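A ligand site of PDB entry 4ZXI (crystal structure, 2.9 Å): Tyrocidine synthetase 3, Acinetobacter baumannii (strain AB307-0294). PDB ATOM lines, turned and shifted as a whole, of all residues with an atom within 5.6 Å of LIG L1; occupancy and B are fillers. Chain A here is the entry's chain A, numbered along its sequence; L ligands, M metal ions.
An oxygen (O2) of LIG L1 is in hydrogen-bond range of the side-chain hydroxyl of Ser 628 (2.4 Å).
An oxygen (O7) of LIG L1 sits at hydrogen-bond distance from the side-chain carboxylate of Asp 851 (2.6 Å).
The backbone carbonyl oxygen (O) of Val 762 sits at hydrogen-bond distance from a nitrogen (N3) of LIG L1, at 2.9 Å.
The guanidinium group (NH2) of Arg 866 lies within salt-bridge range of an oxygen (O2) of LIG L1 (3.9 Å).
OD1 of Asn 761 sits at hydrogen-bond distance from N3 of LIG L1 (3.1 Å).
The backbone NH of Gly 741 sits at hydrogen-bond distance from a nitrogen (N2) of LIG L1.
The side-chain amino group (NZ) of Lys 954 lies within salt-bridge range of an oxygen (O3) of LIG L1 (3.6 Å).
O1 of LIG L1 is in hydrogen-bond range of OG1 of Thr 627 (3.2 Å).
An oxygen (O2) of LG2 L2 is in salt-bridge range of the side-chain amino group of Lys 954 (3.1 Å).
The backbone carbonyl oxygen (O) of Gly 764 sits close to a nitrogen (N1) of LG2 L2 (3.2 Å).
OG1 of Thr 766 lies close to O1 of LG2 L2.
Glu 742 touches LIG L1.
Ala 743 touches LIG L1 (N to C9, 3.7 Å).
Tyr 763 touches LIG L1.
Gly 764 touches LIG L1 (N to N2, 3.9 Å).
Pro 765 touches LIG L1.
Leu 785 touches LIG L1.
His 863 touches LIG L1 (CE1 to N5, 3.6 Å).
Hydrophobic or aromatic side chains that line LIG L1: Tyr 763, Pro 765, Leu 785 and His 863.
Within 4 Å of LIG L1: Thr 627, Ser 628, Gly 741, Glu 742, Ala 743, Asn 761, Val 762, Tyr 763, Gly 764, Pro 765, Leu 785, Asp 851, His 863, Arg 866 and Lys 954.
The nearest printed residue that does not touch LIG L1 is Trp 771 (4.2 Å).
The side-chain amino group of Lys 635 sits at hydrogen-bond distance from the backbone carbonyl oxygen of Ser 628 (3.0 Å).
The side-chain carboxylate (OD1) of Asp 851 is in salt-bridge range of the guanidinium group (NE) of Arg 866.
OG1 of Thr 849 lies within hydrogen-bond range of N of Asp 851.
O of Cys 739 lies within hydrogen-bond range of N of Val 762.
The guanidinium group (NH1) of Arg 866 lies within hydrogen-bond range of the backbone carbonyl oxygen (O) of Thr 849.
The side-chain amide oxygen (OD1) of Asn 761 lies close to the backbone carbonyl oxygen (O) of Cys 739 (3.3 Å).
The backbone carbonyl oxygen (O) of Gly 741 sits close to the side-chain amino group (NZ) of Lys 954 (3.3 Å).
The backbone carbonyl oxygen (O) of Lys 635 is in hydrogen-bond range of the backbone NH (N) of Thr 627 (3.1 Å).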
ATOM      1  N   THR A 627      23.748 -28.477 -28.875  1.00  0.00           N
ATOM      2  CA  THR A 627      24.551 -27.881 -27.820  1.00  0.00           C
ATOM      3  C   THR A 627      25.983 -27.577 -28.258  1.00  0.00           C
ATOM      4  O   THR A 627      26.413 -27.994 -29.349  1.00  0.00           O
ATOM      5  CB  THR A 627      24.600 -28.824 -26.588  1.00  0.00           C
ATOM      6  OG1 THR A 627      25.180 -28.130 -25.474  1.00  0.00           O
ATOM      7  CG2 THR A 627      25.406 -30.091 -26.909  1.00  0.00           C
ATOM      8  N   SER A 628      26.713 -26.846 -27.415  1.00  0.00           N
ATOM      9  CA  SER A 628      28.097 -26.435 -27.649  1.00  0.00           C
ATOM     10  C   SER A 628      29.110 -27.580 -27.520  1.00  0.00           C
ATOM     11  O   SER A 628      29.628 -27.840 -26.424  1.00  0.00           O
ATOM     12  CB  SER A 628      28.480 -25.307 -26.682  1.00  0.00           C
ATOM     13  OG  SER A 628      28.486 -25.767 -25.334  1.00  0.00           O
ATOM     14  N   LYS A 635      26.494 -30.510 -32.170  1.00  0.00           N
ATOM     15  CA  LYS A 635      26.258 -31.721 -31.389  1.00  0.00           C
ATOM     16  C   LYS A 635      24.787 -31.871 -31.032  1.00  0.00           C
ATOM     17  O   LYS A 635      24.305 -31.263 -30.071  1.00  0.00           O
ATOM     18  CB  LYS A 635      27.091 -31.724 -30.102  1.00  0.00           C
ATOM     19  CG  LYS A 635      28.551 -32.114 -30.246  1.00  0.00           C
ATOM     20  CD  LYS A 635      29.233 -32.195 -28.876  1.00  0.00           C
ATOM     21  CE  LYS A 635      29.117 -30.860 -28.153  1.00  0.00           C
ATOM     22  NZ  LYS A 635      29.723 -30.852 -26.802  1.00  0.00           N
ATOM     23  N   CYS A 739      17.757 -22.948  -9.538  1.00  0.00           N
ATOM     24  CA  CYS A 739      18.775 -22.221 -10.266  1.00  0.00           C
ATOM     25  C   CYS A 739      19.783 -23.238 -10.757  1.00  0.00           C
ATOM     26  O   CYS A 739      20.296 -24.047  -9.986  1.00  0.00           O
ATOM     27  CB  CYS A 739      19.420 -21.167  -9.388  1.00  0.00           C
ATOM     28  SG  CYS A 739      20.735 -20.204 -10.157  1.00  0.00           S
ATOM     29  N   GLY A 740      20.040 -23.223 -12.062  1.00  0.00           N
ATOM     30  CA  GLY A 740      20.874 -24.247 -12.686  1.00  0.00           C
ATOM     31  C   GLY A 740      21.475 -23.734 -13.973  1.00  0.00           C
ATOM     32  O   GLY A 740      21.215 -22.595 -14.393  1.00  0.00           O
ATOM     33  N   GLY A 741      22.298 -24.584 -14.598  1.00  0.00           N
ATOM     34  CA  GLY A 741      22.855 -24.305 -15.913  1.00  0.00           C
ATOM     35  C   GLY A 741      24.226 -23.688 -15.794  1.00  0.00           C
ATOM     36  O   GLY A 741      25.008 -23.679 -16.749  1.00  0.00           O
ATOM     37  N   GLU A 742      24.525 -23.181 -14.610  1.00  0.00           N
ATOM     38  CA  GLU A 742      25.678 -22.323 -14.423  1.00  0.00           C
ATOM     39  C   GLU A 742      25.940 -22.211 -12.923  1.00  0.00           C
ATOM     40  O   GLU A 742      25.027 -22.418 -12.098  1.00  0.00           O
ATOM     41  CB  GLU A 742      25.421 -20.942 -15.042  1.00  0.00           C
ATOM     42  CG  GLU A 742      26.658 -20.214 -15.506  1.00  0.00           C
ATOM     43  CD  GLU A 742      26.334 -18.954 -16.323  1.00  0.00           C
ATOM     44  OE1 GLU A 742      25.195 -18.434 -16.230  1.00  0.00           O
ATOM     45  OE2 GLU A 742      27.227 -18.498 -17.066  1.00  0.00           O
ATOM     46  N   ALA A 743      27.175 -21.894 -12.568  1.00  0.00           N
ATOM     47  CA  ALA A 743      27.550 -21.895 -11.164  1.00  0.00           C
ATOM     48  C   ALA A 743      26.818 -20.850 -10.324  1.00  0.00           C
ATOM     49  O   ALA A 743      26.813 -19.645 -10.635  1.00  0.00           O
ATOM     50  CB  ALA A 743      29.025 -21.706 -11.045  1.00  0.00           C
ATOM     51  N   LEU A 744      26.198 -21.321  -9.249  1.00  0.00           N
ATOM     52  CA  LEU A 744      25.572 -20.456  -8.258  1.00  0.00           C
ATOM     53  C   LEU A 744      26.642 -19.902  -7.310  1.00  0.00           C
ATOM     54  O   LEU A 744      27.233 -20.658  -6.525  1.00  0.00           O
ATOM     55  CB  LEU A 744      24.521 -21.241  -7.490  1.00  0.00           C
ATOM     56  CG  LEU A 744      23.823 -20.611  -6.302  1.00  0.00           C
ATOM     57  CD1 LEU A 744      23.082 -19.354  -6.761  1.00  0.00           C
ATOM     58  CD2 LEU A 744      22.863 -21.648  -5.665  1.00  0.00           C
ATOM     59  N   ASN A 761      19.945 -25.591  -5.881  1.00  0.00           N
ATOM     60  CA  ASN A 761      20.971 -25.562  -6.915  1.00  0.00           C
ATOM     61  C   ASN A 761      20.782 -26.823  -7.674  1.00  0.00           C
ATOM     62  O   ASN A 761      20.691 -27.905  -7.069  1.00  0.00           O
ATOM     63  CB  ASN A 761      22.406 -25.480  -6.390  1.00  0.00           C
ATOM     64  CG  ASN A 761      23.432 -25.423  -7.549  1.00  0.00           C
ATOM     65  OD1 ASN A 761      23.046 -25.233  -8.707  1.00  0.00           O
ATOM     66  ND2 ASN A 761      24.724 -25.568  -7.237  1.00  0.00           N
ATOM     67  N   VAL A 762      20.723 -26.730  -8.994  1.00  0.00           N
ATOM     68  CA  VAL A 762      20.458 -27.926  -9.762  1.00  0.00           C
ATOM     69  C   VAL A 762      21.423 -28.018 -10.959  1.00  0.00           C
ATOM     70  O   VAL A 762      21.719 -27.018 -11.617  1.00  0.00           O
ATOM     71  CB  VAL A 762      18.954 -27.971 -10.135  1.00  0.00           C
ATOM     72  CG1 VAL A 762      18.610 -26.998 -11.254  1.00  0.00           C
ATOM     73  CG2 VAL A 762      18.530 -29.354 -10.430  1.00  0.00           C
ATOM     74  N   TYR A 763      21.977 -29.206 -11.180  1.00  0.00           N
ATOM     75  CA  TYR A 763      23.117 -29.385 -12.088  1.00  0.00           C
ATOM     76  C   TYR A 763      22.909 -30.570 -13.021  1.00  0.00           C
ATOM     77  O   TYR A 763      22.311 -31.586 -12.625  1.00  0.00           O
ATOM     78  CB  TYR A 763      24.435 -29.560 -11.293  1.00  0.00           C
ATOM     79  CG  TYR A 763      25.554 -30.216 -12.082  1.00  0.00           C
ATOM     80  CD1 TYR A 763      26.538 -29.457 -12.718  1.00  0.00           C
ATOM     81  CD2 TYR A 763      25.641 -31.611 -12.198  1.00  0.00           C
ATOM     82  CE1 TYR A 763      27.559 -30.067 -13.440  1.00  0.00           C
ATOM     83  CE2 TYR A 763      26.635 -32.219 -12.946  1.00  0.00           C
ATOM     84  CZ  TYR A 763      27.585 -31.451 -13.558  1.00  0.00           C
ATOM     85  OH  TYR A 763      28.572 -32.084 -14.280  1.00  0.00           O
ATOM     86  N   GLY A 764      23.425 -30.458 -14.237  1.00  0.00           N
ATOM     87  CA  GLY A 764      23.465 -31.596 -15.151  1.00  0.00           C
ATOM     88  C   GLY A 764      23.789 -31.210 -16.580  1.00  0.00           C
ATOM     89  O   GLY A 764      23.375 -30.162 -17.043  1.00  0.00           O
ATOM     90  N   PRO A 765      24.542 -32.060 -17.291  1.00  0.00           N
ATOM     91  CA  PRO A 765      24.809 -31.808 -18.695  1.00  0.00           C
ATOM     92  C   PRO A 765      23.628 -32.292 -19.512  1.00  0.00           C
ATOM     93  O   PRO A 765      22.863 -33.117 -19.004  1.00  0.00           O
ATOM     94  CB  PRO A 765      26.054 -32.655 -18.968  1.00  0.00           C
ATOM     95  CG  PRO A 765      25.844 -33.824 -18.116  1.00  0.00           C
ATOM     96  CD  PRO A 765      25.168 -33.318 -16.856  1.00  0.00           C
ATOM     97  N   THR A 766      23.497 -31.809 -20.743  1.00  0.00           N
ATOM     98  CA  THR A 766      22.429 -32.248 -21.636  1.00  0.00           C
ATOM     99  C   THR A 766      22.473 -33.755 -21.918  1.00  0.00           C
ATOM    100  O   THR A 766      21.433 -34.398 -22.110  1.00  0.00           O
ATOM    101  CB  THR A 766      22.489 -31.457 -22.950  1.00  0.00           C
ATOM    102  OG1 THR A 766      22.076 -30.123 -22.693  1.00  0.00           O
ATOM    103  CG2 THR A 766      21.580 -32.040 -24.011  1.00  0.00           C
ATOM    104  N   TRP A 771      18.671 -32.443 -15.610  1.00  0.00           N
ATOM    105  CA  TRP A 771      19.566 -32.405 -14.443  1.00  0.00           C
ATOM    106  C   TRP A 771      19.893 -33.807 -13.993  1.00  0.00           C
ATOM    107  O   TRP A 771      19.101 -34.724 -14.173  1.00  0.00           O
ATOM    108  CB  TRP A 771      18.932 -31.651 -13.264  1.00  0.00           C
ATOM    109  CG  TRP A 771      18.293 -30.318 -13.572  1.00  0.00           C
ATOM    110  CD1 TRP A 771      16.992 -29.988 -13.364  1.00  0.00           C
ATOM    111  CD2 TRP A 771      18.934 -29.144 -14.087  1.00  0.00           C
ATOM    112  NE1 TRP A 771      16.771 -28.693 -13.731  1.00  0.00           N
ATOM    113  CE2 TRP A 771      17.935 -28.148 -14.197  1.00  0.00           C
ATOM    114  CE3 TRP A 771      20.236 -28.834 -14.485  1.00  0.00           C
ATOM    115  CZ2 TRP A 771      18.206 -26.852 -14.671  1.00  0.00           C
ATOM    116  CZ3 TRP A 771      20.501 -27.550 -14.964  1.00  0.00           C
ATOM    117  CH2 TRP A 771      19.486 -26.582 -15.046  1.00  0.00           C
ATOM    118  N   LEU A 785      27.108 -29.302  -5.780  1.00  0.00           N
ATOM    119  CA  LEU A 785      26.272 -29.874  -6.829  1.00  0.00           C
ATOM    120  C   LEU A 785      25.182 -30.776  -6.284  1.00  0.00           C
ATOM    121  O   LEU A 785      24.485 -31.453  -7.051  1.00  0.00           O
ATOM    122  CB  LEU A 785      27.129 -30.641  -7.834  1.00  0.00           C
ATOM    123  CG  LEU A 785      28.149 -29.782  -8.588  1.00  0.00           C
ATOM    124  CD1 LEU A 785      28.884 -30.595  -9.647  1.00  0.00           C
ATOM    125  CD2 LEU A 785      27.471 -28.574  -9.205  1.00  0.00           C
ATOM    126  N   THR A 849      31.811 -35.790 -18.353  1.00  0.00           N
ATOM    127  CA  THR A 849      31.342 -34.404 -18.427  1.00  0.00           C
ATOM    128  C   THR A 849      32.384 -33.380 -18.862  1.00  0.00           C
ATOM    129  O   THR A 849      32.039 -32.348 -19.423  1.00  0.00           O
ATOM    130  CB  THR A 849      30.798 -33.914 -17.084  1.00  0.00           C
ATOM    131  OG1 THR A 849      31.893 -33.682 -16.194  1.00  0.00           O
ATOM    132  CG2 THR A 849      29.872 -34.938 -16.482  1.00  0.00           C
ATOM    133  N   ASP A 851      33.806 -31.725 -16.740  1.00  0.00           N
ATOM    134  CA  ASP A 851      33.691 -30.790 -15.617  1.00  0.00           C
ATOM    135  C   ASP A 851      34.749 -31.042 -14.527  1.00  0.00           C
ATOM    136  O   ASP A 851      35.016 -32.191 -14.157  1.00  0.00           O
ATOM    137  CB  ASP A 851      32.305 -30.850 -14.973  1.00  0.00           C
ATOM    138  CG  ASP A 851      31.277 -30.044 -15.721  1.00  0.00           C
ATOM    139  OD1 ASP A 851      31.666 -29.100 -16.437  1.00  0.00           O
ATOM    140  OD2 ASP A 851      30.075 -30.355 -15.585  1.00  0.00           O
ATOM    141  N   HIS A 863      31.983 -27.576  -7.483  1.00  0.00           N
ATOM    142  CA  HIS A 863      32.269 -27.394  -8.894  1.00  0.00           C
ATOM    143  C   HIS A 863      33.368 -26.351  -9.064  1.00  0.00           C
ATOM    144  O   HIS A 863      33.404 -25.374  -8.329  1.00  0.00           O
ATOM    145  CB  HIS A 863      30.997 -26.972  -9.613  1.00  0.00           C
ATOM    146  CG  HIS A 863      31.174 -26.846 -11.091  1.00  0.00           C
ATOM    147  ND1 HIS A 863      30.833 -27.861 -11.969  1.00  0.00           N
ATOM    148  CD2 HIS A 863      31.676 -25.846 -11.848  1.00  0.00           C
ATOM    149  CE1 HIS A 863      31.106 -27.487 -13.197  1.00  0.00           C
ATOM    150  NE2 HIS A 863      31.618 -26.267 -13.154  1.00  0.00           N
ATOM    151  N   ARG A 866      34.951 -27.040 -15.500  1.00  0.00           N
ATOM    152  CA  ARG A 866      35.437 -27.376 -16.837  1.00  0.00           C
ATOM    153  C   ARG A 866      36.928 -27.672 -16.875  1.00  0.00           C
ATOM    154  O   ARG A 866      37.614 -27.526 -15.874  1.00  0.00           O
ATOM    155  CB  ARG A 866      35.127 -26.234 -17.826  1.00  0.00           C
ATOM    156  CG  ARG A 866      33.679 -26.158 -18.271  1.00  0.00           C
ATOM    157  CD  ARG A 866      33.327 -27.487 -18.854  1.00  0.00           C
ATOM    158  NE  ARG A 866      31.980 -27.521 -19.387  1.00  0.00           N
ATOM    159  CZ  ARG A 866      31.439 -28.613 -19.934  1.00  0.00           C
ATOM    160  NH1 ARG A 866      32.143 -29.731 -19.992  1.00  0.00           N
ATOM    161  NH2 ARG A 866      30.201 -28.576 -20.416  1.00  0.00           N
ATOM    162  N   ASN A 952      21.064 -19.746 -24.541  1.00  0.00           N
ATOM    163  CA  ASN A 952      20.535 -20.339 -23.307  1.00  0.00           C
ATOM    164  C   ASN A 952      20.415 -19.393 -22.120  1.00  0.00           C
ATOM    165  O   ASN A 952      19.914 -19.795 -21.067  1.00  0.00           O
ATOM    166  CB  ASN A 952      21.421 -21.496 -22.833  1.00  0.00           C
ATOM    167  CG  ASN A 952      21.274 -22.728 -23.658  1.00  0.00           C
ATOM    168  OD1 ASN A 952      20.371 -22.850 -24.497  1.00  0.00           O
ATOM    169  ND2 ASN A 952      22.138 -23.709 -23.379  1.00  0.00           N
ATOM    170  N   LYS A 954      23.236 -18.139 -20.543  1.00  0.00           N
ATOM    171  CA  LYS A 954      24.400 -18.316 -19.675  1.00  0.00           C
ATOM    172  C   LYS A 954      25.462 -17.340 -20.127  1.00  0.00           C
ATOM    173  O   LYS A 954      25.410 -16.875 -21.263  1.00  0.00           O
ATOM    174  CB  LYS A 954      24.971 -19.731 -19.736  1.00  0.00           C
ATOM    175  CG  LYS A 954      24.000 -20.853 -19.539  1.00  0.00           C
ATOM    176  CD  LYS A 954      24.770 -22.154 -19.629  1.00  0.00           C
ATOM    177  CE  LYS A 954      23.865 -23.342 -19.551  1.00  0.00           C
ATOM    178  NZ  LYS A 954      24.638 -24.550 -19.906  1.00  0.00           N
HETATM  179  P1  LIG L   1      27.101 -26.407 -22.421  1.00  0.00           P
HETATM  180  O1  LIG L   1      25.734 -26.106 -23.035  1.00  0.00           O
HETATM  181  O2  LIG L   1      28.035 -27.134 -23.383  1.00  0.00           O
HETATM  182  O3  LIG L   1      27.724 -25.263 -21.639  1.00  0.00           O
HETATM  183  O4  LIG L   1      26.818 -27.549 -21.329  1.00  0.00           O
HETATM  184  C1  LIG L   1      26.190 -27.271 -20.070  1.00  0.00           C
HETATM  185  C2  LIG L   1      27.164 -27.337 -18.911  1.00  0.00           C
HETATM  186  O5  LIG L   1      26.788 -26.399 -17.885  1.00  0.00           O
HETATM  187  C3  LIG L   1      27.267 -28.641 -18.137  1.00  0.00           C
HETATM  188  O6  LIG L   1      28.011 -29.648 -18.796  1.00  0.00           O
HETATM  189  C4  LIG L   1      27.926 -28.199 -16.830  1.00  0.00           C
HETATM  190  O7  LIG L   1      29.331 -28.146 -16.973  1.00  0.00           O
HETATM  191  C5  LIG L   1      27.416 -26.763 -16.678  1.00  0.00           C
HETATM  192  N1  LIG L   1      26.451 -26.656 -15.576  1.00  0.00           N
HETATM  193  C6  LIG L   1      25.140 -26.964 -15.623  1.00  0.00           C
HETATM  194  N2  LIG L   1      24.547 -26.761 -14.422  1.00  0.00           N
HETATM  195  C7  LIG L   1      25.499 -26.327 -13.581  1.00  0.00           C
HETATM  196  C8  LIG L   1      25.545 -25.954 -12.145  1.00  0.00           C
HETATM  197  N3  LIG L   1      24.437 -25.989 -11.354  1.00  0.00           N
HETATM  198  N4  LIG L   1      26.749 -25.567 -11.647  1.00  0.00           N
HETATM  199  C9  LIG L   1      27.849 -25.534 -12.423  1.00  0.00           C
HETATM  200  N5  LIG L   1      27.878 -25.876 -13.727  1.00  0.00           N
HETATM  201  C10 LIG L   1      26.746 -26.272 -14.346  1.00  0.00           C
HETATM  202  N1  LG2 L   2      21.032 -29.818 -19.229  1.00  0.00           N
HETATM  203  C1  LG2 L   2      21.346 -28.556 -18.583  1.00  0.00           C
HETATM  204  C2  LG2 L   2      22.592 -27.846 -19.116  1.00  0.00           C
HETATM  205  O1  LG2 L   2      23.172 -28.226 -20.134  1.00  0.00           O
HETATM  206  O2  LG2 L   2      23.058 -26.848 -18.535  1.00  0.00           O
HETATM  207 MG    MG M   1      24.402 -28.658 -21.597  1.00  0.00          MG
